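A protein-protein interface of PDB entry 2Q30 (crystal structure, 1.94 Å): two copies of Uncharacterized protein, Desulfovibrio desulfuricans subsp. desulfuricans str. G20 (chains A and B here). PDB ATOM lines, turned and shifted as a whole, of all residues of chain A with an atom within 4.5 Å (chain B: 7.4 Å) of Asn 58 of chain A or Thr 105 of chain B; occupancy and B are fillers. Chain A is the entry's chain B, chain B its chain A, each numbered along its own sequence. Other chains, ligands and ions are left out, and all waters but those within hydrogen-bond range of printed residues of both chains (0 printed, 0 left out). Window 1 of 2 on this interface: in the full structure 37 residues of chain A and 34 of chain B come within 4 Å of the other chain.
OG1 of Thr 105 of chain A sits at hydrogen-bond distance from ND2 of Asn 58 of chain B (3.2 Å).
The side-chain hydroxyl (OG1) of Thr 105 of chain B is in hydrogen-bond range of the side-chain amide nitrogen (ND2) of Asn 58 of chain A, at 3.2 Å.
The backbone carbonyl oxygen of Thr 105 of chain B sits at hydrogen-bond distance from the backbone NH of Asn 58 of chain B, 2.9 Å away.
O of Thr 105 of chain A lies within hydrogen-bond range of N of Asn 58 of chain A, 2.9 Å away.
N of Glu 56 of chain B sits at hydrogen-bond distance from O of Ala 107 of chain B (2.9 Å).
The backbone NH (N) of Val 60 of chain B is in hydrogen-bond range of the backbone carbonyl oxygen (O) of Leu 103 of chain B, at 2.8 Å.
O of His 28 of chain B lies within hydrogen-bond range of N of Ile 35 of chain B.
N of Leu 57 of chain B is in hydrogen-bond range of O of Ala 86 of chain B.
CZ of Phe 33 of chain A touches C of Leu 57 of chain B, 3.7 Å away.
Phe 33 of chain A touches Asn 58 of chain B.
Phe 33 of chain A touches Ala 107 of chain B (CD2 to CB, 3.7 Å).
Asn 58 of chain A touches Phe 33 of chain B.
Asn 58 of chain A touches Ile 35 of chain B.
CG2 of Val 60 of chain A touches CD2 of Leu 103 of chain B, 3.6 Å away.
His 28 of chain B touches Val 85 of chain A (NE2 to CG1, 3.6 Å).
Val 85 of chain A touches Phe 33 of chain B (CG1 to CE1, 3.8 Å).
CD1 of Ile 35 of chain B touches CG2 of Val 85 of chain A, at 3.7 Å.
Leu 103 of chain A touches Val 60 of chain B.
Asn 58 of chain A touches three residues of chain B.
Printed residues of chain A within 4 Å of Thr 105 of chain B: Phe 33, Asn 58 and Thr 105.
Of the printed residues of chain B, Phe 33 of chain A touches Glu 56 (3.5 Å), Leu 57 (3.7 Å), Asn 58 (3.7 Å), Thr 105 (3.8 Å) and Ala 107 (3.7 Å).
Of the printed residues of chain A, Glu 56 of chain B touches Phe 33 (3.5 Å).
Printed residues of chain A within 4 Å of Leu 57 of chain B: Phe 33 (3.7 Å).
Printed residues of chain B within 4 Å of Leu 57 of chain A: Phe 33 (3.7 Å).
Of the printed residues of chain A, Ile 35 of chain B touches Asn 58 (3.3 Å) and Val 85 (3.7 Å).
Val 83 of chain A touches none of the printed residues of chain B.
The nearest printed residue of chain A that does not touch Leu 57 of chain B is Thr 105 of chain A (7.6 Å).
Of the 11 printed residues of chain A, 7 touch a printed residue of chain B.
Hydrophobic or aromatic side chains of chain A that line the printed part of chain B: Phe 33, Val 60, Val 85 and Leu 103.
Printed residues of chain B that touch a printed residue of chain A: His 28, Phe 33, Ile 35, Glu 56, Leu 57, Asn 58, Val 60, Leu 103, Thr 105 and Ala 107.
Among the printed residues, no Asp or Glu carboxylate lies within 4 Å of a Lys or Arg side-chain nitrogen of the other chain.
Phe 33 of chain A touches Leu 57 of chain B, and with the chains exchanged Leu 57 of chain A touches Phe 33 of chain B.
Phe 33 of chain A touches Asn 58 of chain B, and with the chains exchanged Asn 58 of chain A touches Phe 33 of chain B.
Asn 58 of chain A touches Thr 105 of chain B, and with the chains exchanged Thr 105 of chain A touches Asn 58 of chain B.
Val 60 of chain A touches Leu 103 of chain B, and with the chains exchanged Leu 103 of chain A touches Val 60 of chain B.
Positions printed for both chains: 33, 57, 58, 59, 60, 84, 103, 104 and 105.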
ATOM      1  N   PHE A  33      -9.594  -4.826  19.710  1.00  0.00           N
ATOM      2  CA  PHE A  33      -8.931  -4.806  20.988  1.00  0.00           C
ATOM      3  C   PHE A  33      -8.766  -3.379  21.548  1.00  0.00           C
ATOM      4  O   PHE A  33      -8.904  -2.382  20.829  1.00  0.00           O
ATOM      5  CB  PHE A  33      -7.554  -5.561  20.979  1.00  0.00           C
ATOM      6  CG  PHE A  33      -6.578  -5.210  19.826  1.00  0.00           C
ATOM      7  CD1 PHE A  33      -6.581  -3.985  19.149  1.00  0.00           C
ATOM      8  CD2 PHE A  33      -5.564  -6.119  19.509  1.00  0.00           C
ATOM      9  CE1 PHE A  33      -5.645  -3.714  18.132  1.00  0.00           C
ATOM     10  CE2 PHE A  33      -4.620  -5.846  18.527  1.00  0.00           C
ATOM     11  CZ  PHE A  33      -4.666  -4.643  17.827  1.00  0.00           C
ATOM     12  N   LEU A  57      -6.623 -10.996  28.100  1.00  0.00           N
ATOM     13  CA  LEU A  57      -5.747  -9.837  28.042  1.00  0.00           C
ATOM     14  C   LEU A  57      -4.331 -10.352  28.044  1.00  0.00           C
ATOM     15  O   LEU A  57      -4.089 -11.488  28.489  1.00  0.00           O
ATOM     16  CB  LEU A  57      -5.960  -8.877  29.226  1.00  0.00           C
ATOM     17  CG  LEU A  57      -5.553  -9.270  30.658  1.00  0.00           C
ATOM     18  CD1 LEU A  57      -5.293  -8.028  31.489  1.00  0.00           C
ATOM     19  CD2 LEU A  57      -6.565 -10.156  31.351  1.00  0.00           C
ATOM     20  N   ASN A  58      -3.403  -9.541  27.525  1.00  0.00           N
ATOM     21  CA  ASN A  58      -1.989  -9.829  27.731  1.00  0.00           C
ATOM     22  C   ASN A  58      -1.366  -8.561  28.332  1.00  0.00           C
ATOM     23  O   ASN A  58      -1.795  -7.459  28.003  1.00  0.00           O
ATOM     24  CB  ASN A  58      -1.267 -10.431  26.505  1.00  0.00           C
ATOM     25  CG  ASN A  58      -0.967  -9.433  25.390  1.00  0.00           C
ATOM     26  OD1 ASN A  58      -0.223  -8.491  25.570  1.00  0.00           O
ATOM     27  ND2 ASN A  58      -1.463  -9.715  24.205  1.00  0.00           N
ATOM     28  N   ILE A  59      -0.379  -8.727  29.196  1.00  0.00           N
ATOM     29  CA  ILE A  59       0.307  -7.609  29.823  1.00  0.00           C
ATOM     30  C   ILE A  59       1.768  -7.810  29.502  1.00  0.00           C
ATOM     31  O   ILE A  59       2.325  -8.832  29.883  1.00  0.00           O
ATOM     32  CB  ILE A  59       0.103  -7.584  31.321  1.00  0.00           C
ATOM     33  CG1 ILE A  59      -1.394  -7.655  31.661  1.00  0.00           C
ATOM     34  CG2 ILE A  59       0.804  -6.334  31.932  1.00  0.00           C
ATOM     35  CD1 ILE A  59      -1.665  -7.708  33.155  1.00  0.00           C
ATOM     36  N   VAL A  60       2.374  -6.822  28.838  1.00  0.00           N
ATOM     37  CA  VAL A  60       3.767  -6.867  28.396  1.00  0.00           C
ATOM     38  C   VAL A  60       4.533  -5.831  29.183  1.00  0.00           C
ATOM     39  O   VAL A  60       4.130  -4.678  29.208  1.00  0.00           O
ATOM     40  CB  VAL A  60       3.924  -6.573  26.870  1.00  0.00           C
ATOM     41  CG1 VAL A  60       5.407  -6.679  26.471  1.00  0.00           C
ATOM     42  CG2 VAL A  60       3.084  -7.577  26.036  1.00  0.00           C
ATOM     43  N   VAL A  83       5.542 -11.415  29.484  1.00  0.00           N
ATOM     44  CA  VAL A  83       4.178 -11.270  29.009  1.00  0.00           C
ATOM     45  C   VAL A  83       3.291 -12.191  29.815  1.00  0.00           C
ATOM     46  O   VAL A  83       3.585 -13.373  29.917  1.00  0.00           O
ATOM     47  CB  VAL A  83       4.016 -11.532  27.476  1.00  0.00           C
ATOM     48  CG1 VAL A  83       4.454 -12.892  27.075  1.00  0.00           C
ATOM     49  CG2 VAL A  83       2.567 -11.290  27.026  1.00  0.00           C
ATOM     50  N   LEU A  84       2.230 -11.630  30.387  1.00  0.00           N
ATOM     51  CA  LEU A  84       1.201 -12.370  31.075  1.00  0.00           C
ATOM     52  C   LEU A  84       0.048 -12.490  30.096  1.00  0.00           C
ATOM     53  O   LEU A  84      -0.321 -11.507  29.446  1.00  0.00           O
ATOM     54  CB  LEU A  84       0.682 -11.601  32.299  1.00  0.00           C
ATOM     55  CG  LEU A  84      -0.466 -12.270  33.074  1.00  0.00           C
ATOM     56  CD1 LEU A  84       0.123 -13.381  33.961  1.00  0.00           C
ATOM     57  CD2 LEU A  84      -1.231 -11.273  33.949  1.00  0.00           C
ATOM     58  N   VAL A  85      -0.498 -13.688  29.954  1.00  0.00           N
ATOM     59  CA  VAL A  85      -1.735 -13.879  29.189  1.00  0.00           C
ATOM     60  C   VAL A  85      -2.713 -14.472  30.194  1.00  0.00           C
ATOM     61  O   VAL A  85      -2.381 -15.427  30.885  1.00  0.00           O
ATOM     62  CB  VAL A  85      -1.584 -14.808  27.994  1.00  0.00           C
ATOM     63  CG1 VAL A  85      -2.942 -14.866  27.209  1.00  0.00           C
ATOM     64  CG2 VAL A  85      -0.418 -14.378  27.109  1.00  0.00           C
ATOM     65  N   LEU A 103       2.252  -2.600  28.858  1.00  0.00           N
ATOM     66  CA  LEU A 103       1.277  -2.440  27.791  1.00  0.00           C
ATOM     67  C   LEU A 103       0.282  -3.575  27.917  1.00  0.00           C
ATOM     68  O   LEU A 103       0.670  -4.741  27.975  1.00  0.00           O
ATOM     69  CB  LEU A 103       1.962  -2.487  26.433  1.00  0.00           C
ATOM     70  CG  LEU A 103       1.075  -2.157  25.216  1.00  0.00           C
ATOM     71  CD1 LEU A 103       0.591  -0.768  25.285  1.00  0.00           C
ATOM     72  CD2 LEU A 103       1.897  -2.335  23.961  1.00  0.00           C
ATOM     73  N   VAL A 104      -1.005  -3.237  27.962  1.00  0.00           N
ATOM     74  CA  VAL A 104      -2.065  -4.217  28.105  1.00  0.00           C
ATOM     75  C   VAL A 104      -2.942  -4.197  26.878  1.00  0.00           C
ATOM     76  O   VAL A 104      -3.361  -3.141  26.452  1.00  0.00           O
ATOM     77  CB  VAL A 104      -2.936  -3.964  29.339  1.00  0.00           C
ATOM     78  CG1 VAL A 104      -3.963  -5.034  29.444  1.00  0.00           C
ATOM     79  CG2 VAL A 104      -2.098  -3.937  30.596  1.00  0.00           C
ATOM     80  N   THR A 105      -3.151  -5.367  26.288  1.00  0.00           N
ATOM     81  CA  THR A 105      -4.019  -5.547  25.135  1.00  0.00           C
ATOM     82  C   THR A 105      -5.146  -6.432  25.608  1.00  0.00           C
ATOM     83  O   THR A 105      -4.865  -7.491  26.143  1.00  0.00           O
ATOM     84  CB  THR A 105      -3.276  -6.227  24.011  1.00  0.00           C
ATOM     85  OG1 THR A 105      -2.247  -5.341  23.575  1.00  0.00           O
ATOM     86  CG2 THR A 105      -4.218  -6.536  22.835  1.00  0.00           C
ATOM     87  N   HIS B  28       1.166 -17.582  22.224  1.00  0.00           N
ATOM     88  CA  HIS B  28      -0.183 -17.958  22.625  1.00  0.00           C
ATOM     89  C   HIS B  28      -1.121 -17.941  21.420  1.00  0.00           C
ATOM     90  O   HIS B  28      -0.941 -17.144  20.475  1.00  0.00           O
ATOM     91  CB  HIS B  28      -0.655 -16.959  23.689  1.00  0.00           C
ATOM     92  CG  HIS B  28      -2.016 -17.225  24.232  1.00  0.00           C
ATOM     93  ND1 HIS B  28      -2.250 -18.146  25.230  1.00  0.00           N
ATOM     94  CD2 HIS B  28      -3.212 -16.673  23.936  1.00  0.00           C
ATOM     95  CE1 HIS B  28      -3.536 -18.150  25.529  1.00  0.00           C
ATOM     96  NE2 HIS B  28      -4.143 -17.271  24.753  1.00  0.00           N
ATOM     97  N   ASN B  32      -9.497 -15.656  21.048  1.00  0.00           N
ATOM     98  CA  ASN B  32      -9.445 -14.209  21.251  1.00  0.00           C
ATOM     99  C   ASN B  32      -8.297 -13.499  20.552  1.00  0.00           C
ATOM    100  O   ASN B  32      -8.486 -12.431  19.966  1.00  0.00           O
ATOM    101  CB  ASN B  32      -9.403 -13.924  22.747  1.00  0.00           C
ATOM    102  CG  ASN B  32     -10.575 -14.525  23.479  1.00  0.00           C
ATOM    103  OD1 ASN B  32     -11.713 -14.294  23.107  1.00  0.00           O
ATOM    104  ND2 ASN B  32     -10.307 -15.318  24.508  1.00  0.00           N
ATOM    105  N   PHE B  33      -7.098 -14.064  20.649  1.00  0.00           N
ATOM    106  CA  PHE B  33      -5.945 -13.554  19.918  1.00  0.00           C
ATOM    107  C   PHE B  33      -4.834 -14.588  19.685  1.00  0.00           C
ATOM    108  O   PHE B  33      -4.821 -15.664  20.279  1.00  0.00           O
ATOM    109  CB  PHE B  33      -5.365 -12.253  20.543  1.00  0.00           C
ATOM    110  CG  PHE B  33      -5.207 -12.260  22.064  1.00  0.00           C
ATOM    111  CD1 PHE B  33      -4.976 -13.431  22.813  1.00  0.00           C
ATOM    112  CD2 PHE B  33      -5.202 -11.035  22.748  1.00  0.00           C
ATOM    113  CE1 PHE B  33      -4.803 -13.363  24.207  1.00  0.00           C
ATOM    114  CE2 PHE B  33      -5.011 -10.978  24.144  1.00  0.00           C
ATOM    115  CZ  PHE B  33      -4.818 -12.150  24.857  1.00  0.00           C
ATOM    116  N   LYS B  34      -3.919 -14.230  18.790  1.00  0.00           N
ATOM    117  CA  LYS B  34      -2.707 -14.988  18.518  1.00  0.00           C
ATOM    118  C   LYS B  34      -1.578 -14.048  18.881  1.00  0.00           C
ATOM    119  O   LYS B  34      -1.624 -12.869  18.522  1.00  0.00           O
ATOM    120  CB  LYS B  34      -2.615 -15.411  17.051  1.00  0.00           C
ATOM    121  CG  LYS B  34      -1.360 -16.218  16.715  1.00  0.00           C
ATOM    122  CD  LYS B  34      -1.457 -16.732  15.283  1.00  0.00           C
ATOM    123  CE  LYS B  34      -0.314 -17.606  14.894  1.00  0.00           C
ATOM    124  NZ  LYS B  34      -0.504 -18.129  13.499  1.00  0.00           N
ATOM    125  N   ILE B  35      -0.619 -14.560  19.636  1.00  0.00           N
ATOM    126  CA  ILE B  35       0.513 -13.812  20.108  1.00  0.00           C
ATOM    127  C   ILE B  35       1.742 -14.572  19.627  1.00  0.00           C
ATOM    128  O   ILE B  35       1.915 -15.756  19.971  1.00  0.00           O
ATOM    129  CB  ILE B  35       0.511 -13.676  21.643  1.00  0.00           C
ATOM    130  CG1 ILE B  35      -0.814 -13.115  22.150  1.00  0.00           C
ATOM    131  CG2 ILE B  35       1.659 -12.777  22.090  1.00  0.00           C
ATOM    132  CD1 ILE B  35      -0.909 -12.976  23.714  1.00  0.00           C
ATOM    133  N   VAL B  36       2.585 -13.895  18.844  1.00  0.00           N
ATOM    134  CA  VAL B  36       3.811 -14.478  18.306  1.00  0.00           C
ATOM    135  C   VAL B  36       4.967 -13.493  18.391  1.00  0.00           C
ATOM    136  O   VAL B  36       4.775 -12.272  18.251  1.00  0.00           O
ATOM    137  CB  VAL B  36       3.617 -14.921  16.828  1.00  0.00           C
ATOM    138  CG1 VAL B  36       2.759 -16.159  16.768  1.00  0.00           C
ATOM    139  CG2 VAL B  36       3.020 -13.785  15.983  1.00  0.00           C
ATOM    140  N   SER B  37       6.158 -14.025  18.630  1.00  0.00           N
ATOM    141  CA  SER B  37       7.354 -13.226  18.722  1.00  0.00           C
ATOM    142  C   SER B  37       8.184 -13.458  17.475  1.00  0.00           C
ATOM    143  O   SER B  37       8.069 -14.508  16.828  1.00  0.00           O
ATOM    144  CB  SER B  37       8.169 -13.538  19.969  1.00  0.00           C
ATOM    145  OG  SER B  37       8.703 -14.830  19.951  1.00  0.00           O
ATOM    146  N   GLU B  56      -7.046  -6.477  13.670  1.00  0.00           N
ATOM    147  CA  GLU B  56      -5.843  -5.668  13.794  1.00  0.00           C
ATOM    148  C   GLU B  56      -4.686  -6.400  14.440  1.00  0.00           C
ATOM    149  O   GLU B  56      -4.865  -7.448  15.022  1.00  0.00           O
ATOM    150  CB  GLU B  56      -6.187  -4.442  14.632  1.00  0.00           C
ATOM    151  CG  GLU B  56      -6.994  -3.406  13.886  1.00  0.00           C
ATOM    152  CD  GLU B  56      -7.608  -2.416  14.831  1.00  0.00           C
ATOM    153  OE1 GLU B  56      -8.590  -2.793  15.488  1.00  0.00           O
ATOM    154  OE2 GLU B  56      -7.148  -1.257  14.882  1.00  0.00           O
ATOM    155  N   LEU B  57      -3.487  -5.850  14.300  1.00  0.00           N
ATOM    156  CA  LEU B  57      -2.351  -6.361  15.055  1.00  0.00           C
ATOM    157  C   LEU B  57      -1.660  -5.221  15.754  1.00  0.00           C
ATOM    158  O   LEU B  57      -1.779  -4.068  15.335  1.00  0.00           O
ATOM    159  CB  LEU B  57      -1.320  -7.111  14.202  1.00  0.00           C
ATOM    160  CG  LEU B  57      -0.458  -6.314  13.201  1.00  0.00           C
ATOM    161  CD1 LEU B  57       0.774  -7.095  12.820  1.00  0.00           C
ATOM    162  CD2 LEU B  57      -1.259  -5.965  11.997  1.00  0.00           C
ATOM    163  N   ASN B  58      -0.927  -5.549  16.815  1.00  0.00           N
ATOM    164  CA  ASN B  58      -0.020  -4.576  17.395  1.00  0.00           C
ATOM    165  C   ASN B  58       1.345  -5.260  17.438  1.00  0.00           C
ATOM    166  O   ASN B  58       1.416  -6.477  17.664  1.00  0.00           O
ATOM    167  CB  ASN B  58      -0.523  -3.960  18.710  1.00  0.00           C
ATOM    168  CG  ASN B  58      -0.387  -4.872  19.914  1.00  0.00           C
ATOM    169  OD1 ASN B  58       0.695  -5.119  20.397  1.00  0.00           O
ATOM    170  ND2 ASN B  58      -1.503  -5.274  20.456  1.00  0.00           N
ATOM    171  N   ILE B  59       2.396  -4.506  17.171  1.00  0.00           N
ATOM    172  CA  ILE B  59       3.761  -5.013  17.202  1.00  0.00           C
ATOM    173  C   ILE B  59       4.486  -4.196  18.256  1.00  0.00           C
ATOM    174  O   ILE B  59       4.622  -2.990  18.083  1.00  0.00           O
ATOM    175  CB  ILE B  59       4.488  -4.868  15.867  1.00  0.00           C
ATOM    176  CG1 ILE B  59       3.706  -5.556  14.748  1.00  0.00           C
ATOM    177  CG2 ILE B  59       5.925  -5.405  16.002  1.00  0.00           C
ATOM    178  CD1 ILE B  59       4.366  -5.519  13.370  1.00  0.00           C
ATOM    179  N   VAL B  60       4.975  -4.855  19.307  1.00  0.00           N
ATOM    180  CA  VAL B  60       5.670  -4.186  20.401  1.00  0.00           C
ATOM    181  C   VAL B  60       7.152  -4.526  20.351  1.00  0.00           C
ATOM    182  O   VAL B  60       7.500  -5.690  20.320  1.00  0.00           O
ATOM    183  CB  VAL B  60       5.103  -4.647  21.759  1.00  0.00           C
ATOM    184  CG1 VAL B  60       5.773  -3.834  22.899  1.00  0.00           C
ATOM    185  CG2 VAL B  60       3.593  -4.453  21.758  1.00  0.00           C
ATOM    186  N   LEU B  84       3.442  -0.562  17.102  1.00  0.00           N
ATOM    187  CA  LEU B  84       2.765  -0.272  15.847  1.00  0.00           C
ATOM    188  C   LEU B  84       1.404  -0.906  15.989  1.00  0.00           C
ATOM    189  O   LEU B  84       1.354  -2.023  16.457  1.00  0.00           O
ATOM    190  CB  LEU B  84       3.479  -0.964  14.701  1.00  0.00           C
ATOM    191  CG  LEU B  84       2.853  -0.877  13.301  1.00  0.00           C
ATOM    192  CD1 LEU B  84       2.969   0.508  12.748  1.00  0.00           C
ATOM    193  CD2 LEU B  84       3.568  -1.898  12.423  1.00  0.00           C
ATOM    194  N   ALA B  86      -2.019  -1.683  13.541  1.00  0.00           N
ATOM    195  CA  ALA B  86      -2.452  -1.673  12.162  1.00  0.00           C
ATOM    196  C   ALA B  86      -3.483  -2.736  11.878  1.00  0.00           C
ATOM    197  O   ALA B  86      -3.518  -3.750  12.572  1.00  0.00           O
ATOM    198  CB  ALA B  86      -1.221  -1.885  11.227  1.00  0.00           C
ATOM    199  N   ILE B  88      -4.762  -5.935  10.013  1.00  0.00           N
ATOM    200  CA  ILE B  88      -4.061  -7.122   9.495  1.00  0.00           C
ATOM    201  C   ILE B  88      -3.903  -7.065   7.955  1.00  0.00           C
ATOM    202  O   ILE B  88      -2.905  -7.564   7.398  1.00  0.00           O
ATOM    203  CB  ILE B  88      -4.808  -8.427   9.931  1.00  0.00           C
ATOM    204  CG1 ILE B  88      -4.741  -8.613  11.448  1.00  0.00           C
ATOM    205  CG2 ILE B  88      -4.230  -9.663   9.280  1.00  0.00           C
ATOM    206  CD1 ILE B  88      -5.764  -9.642  11.939  1.00  0.00           C
ATOM    207  N   LEU B 103       7.000  -8.520  19.777  1.00  0.00           N
ATOM    208  CA  LEU B 103       5.841  -9.336  20.110  1.00  0.00           C
ATOM    209  C   LEU B 103       4.683  -8.828  19.293  1.00  0.00           C
ATOM    210  O   LEU B 103       4.402  -7.642  19.294  1.00  0.00           O
ATOM    211  CB  LEU B 103       5.504  -9.212  21.592  1.00  0.00           C
ATOM    212  CG  LEU B 103       4.450 -10.215  22.093  1.00  0.00           C
ATOM    213  CD1 LEU B 103       4.903 -11.673  21.896  1.00  0.00           C
ATOM    214  CD2 LEU B 103       4.178  -9.938  23.580  1.00  0.00           C
ATOM    215  N   VAL B 104       4.004  -9.739  18.619  1.00  0.00           N
ATOM    216  CA  VAL B 104       2.874  -9.405  17.790  1.00  0.00           C
ATOM    217  C   VAL B 104       1.645 -10.036  18.393  1.00  0.00           C
ATOM    218  O   VAL B 104       1.675 -11.207  18.672  1.00  0.00           O
ATOM    219  CB  VAL B 104       3.084  -9.928  16.346  1.00  0.00           C
ATOM    220  CG1 VAL B 104       1.854  -9.568  15.442  1.00  0.00           C
ATOM    221  CG2 VAL B 104       4.374  -9.369  15.785  1.00  0.00           C
ATOM    222  N   THR B 105       0.585  -9.245  18.576  1.00  0.00           N
ATOM    223  CA  THR B 105      -0.728  -9.684  19.056  1.00  0.00           C
ATOM    224  C   THR B 105      -1.715  -9.349  17.941  1.00  0.00           C
ATOM    225  O   THR B 105      -1.786  -8.202  17.502  1.00  0.00           O
ATOM    226  CB  THR B 105      -1.149  -8.999  20.370  1.00  0.00           C
ATOM    227  OG1 THR B 105      -0.144  -9.285  21.358  1.00  0.00           O
ATOM    228  CG2 THR B 105      -2.513  -9.551  20.839  1.00  0.00           C
ATOM    229  N   ILE B 106      -2.441 -10.358  17.497  1.00  0.00           N
ATOM    230  CA  ILE B 106      -3.369 -10.290  16.374  1.00  0.00           C
ATOM    231  C   ILE B 106      -4.748 -10.640  16.909  1.00  0.00           C
ATOM    232  O   ILE B 106      -4.895 -11.696  17.505  1.00  0.00           O
ATOM    233  CB  ILE B 106      -2.956 -11.302  15.277  1.00  0.00           C
ATOM    234  CG1 ILE B 106      -1.448 -11.183  14.940  1.00  0.00           C
ATOM    235  CG2 ILE B 106      -3.828 -11.113  14.057  1.00  0.00           C
ATOM    236  CD1 ILE B 106      -0.933 -12.305  14.051  1.00  0.00           C
ATOM    237  N   ALA B 107      -5.731  -9.754  16.709  1.00  0.00           N
ATOM    238  CA  ALA B 107      -7.121  -9.941  17.197  1.00  0.00           C
ATOM    239  C   ALA B 107      -8.172  -9.430  16.199  1.00  0.00           C
ATOM    240  O   ALA B 107      -8.019  -8.331  15.671  1.00  0.00           O
ATOM    241  CB  ALA B 107      -7.331  -9.246  18.507  1.00  0.00           C
ATOM    242  N   PRO B 108      -9.149 -10.278  15.819  1.00  0.00           N
ATOM    243  CA  PRO B 108      -9.251 -11.707  16.124  1.00  0.00           C
ATOM    244  C   PRO B 108      -8.074 -12.464  15.461  1.00  0.00           C
ATOM    245  O   PRO B 108      -7.407 -11.896  14.590  1.00  0.00           O
ATOM    246  CB  PRO B 108     -10.581 -12.125  15.486  1.00  0.00           C
ATOM    247  CG  PRO B 108     -11.345 -10.839  15.318  1.00  0.00           C
ATOM    248  CD  PRO B 108     -10.292  -9.817  15.016  1.00  0.00           C
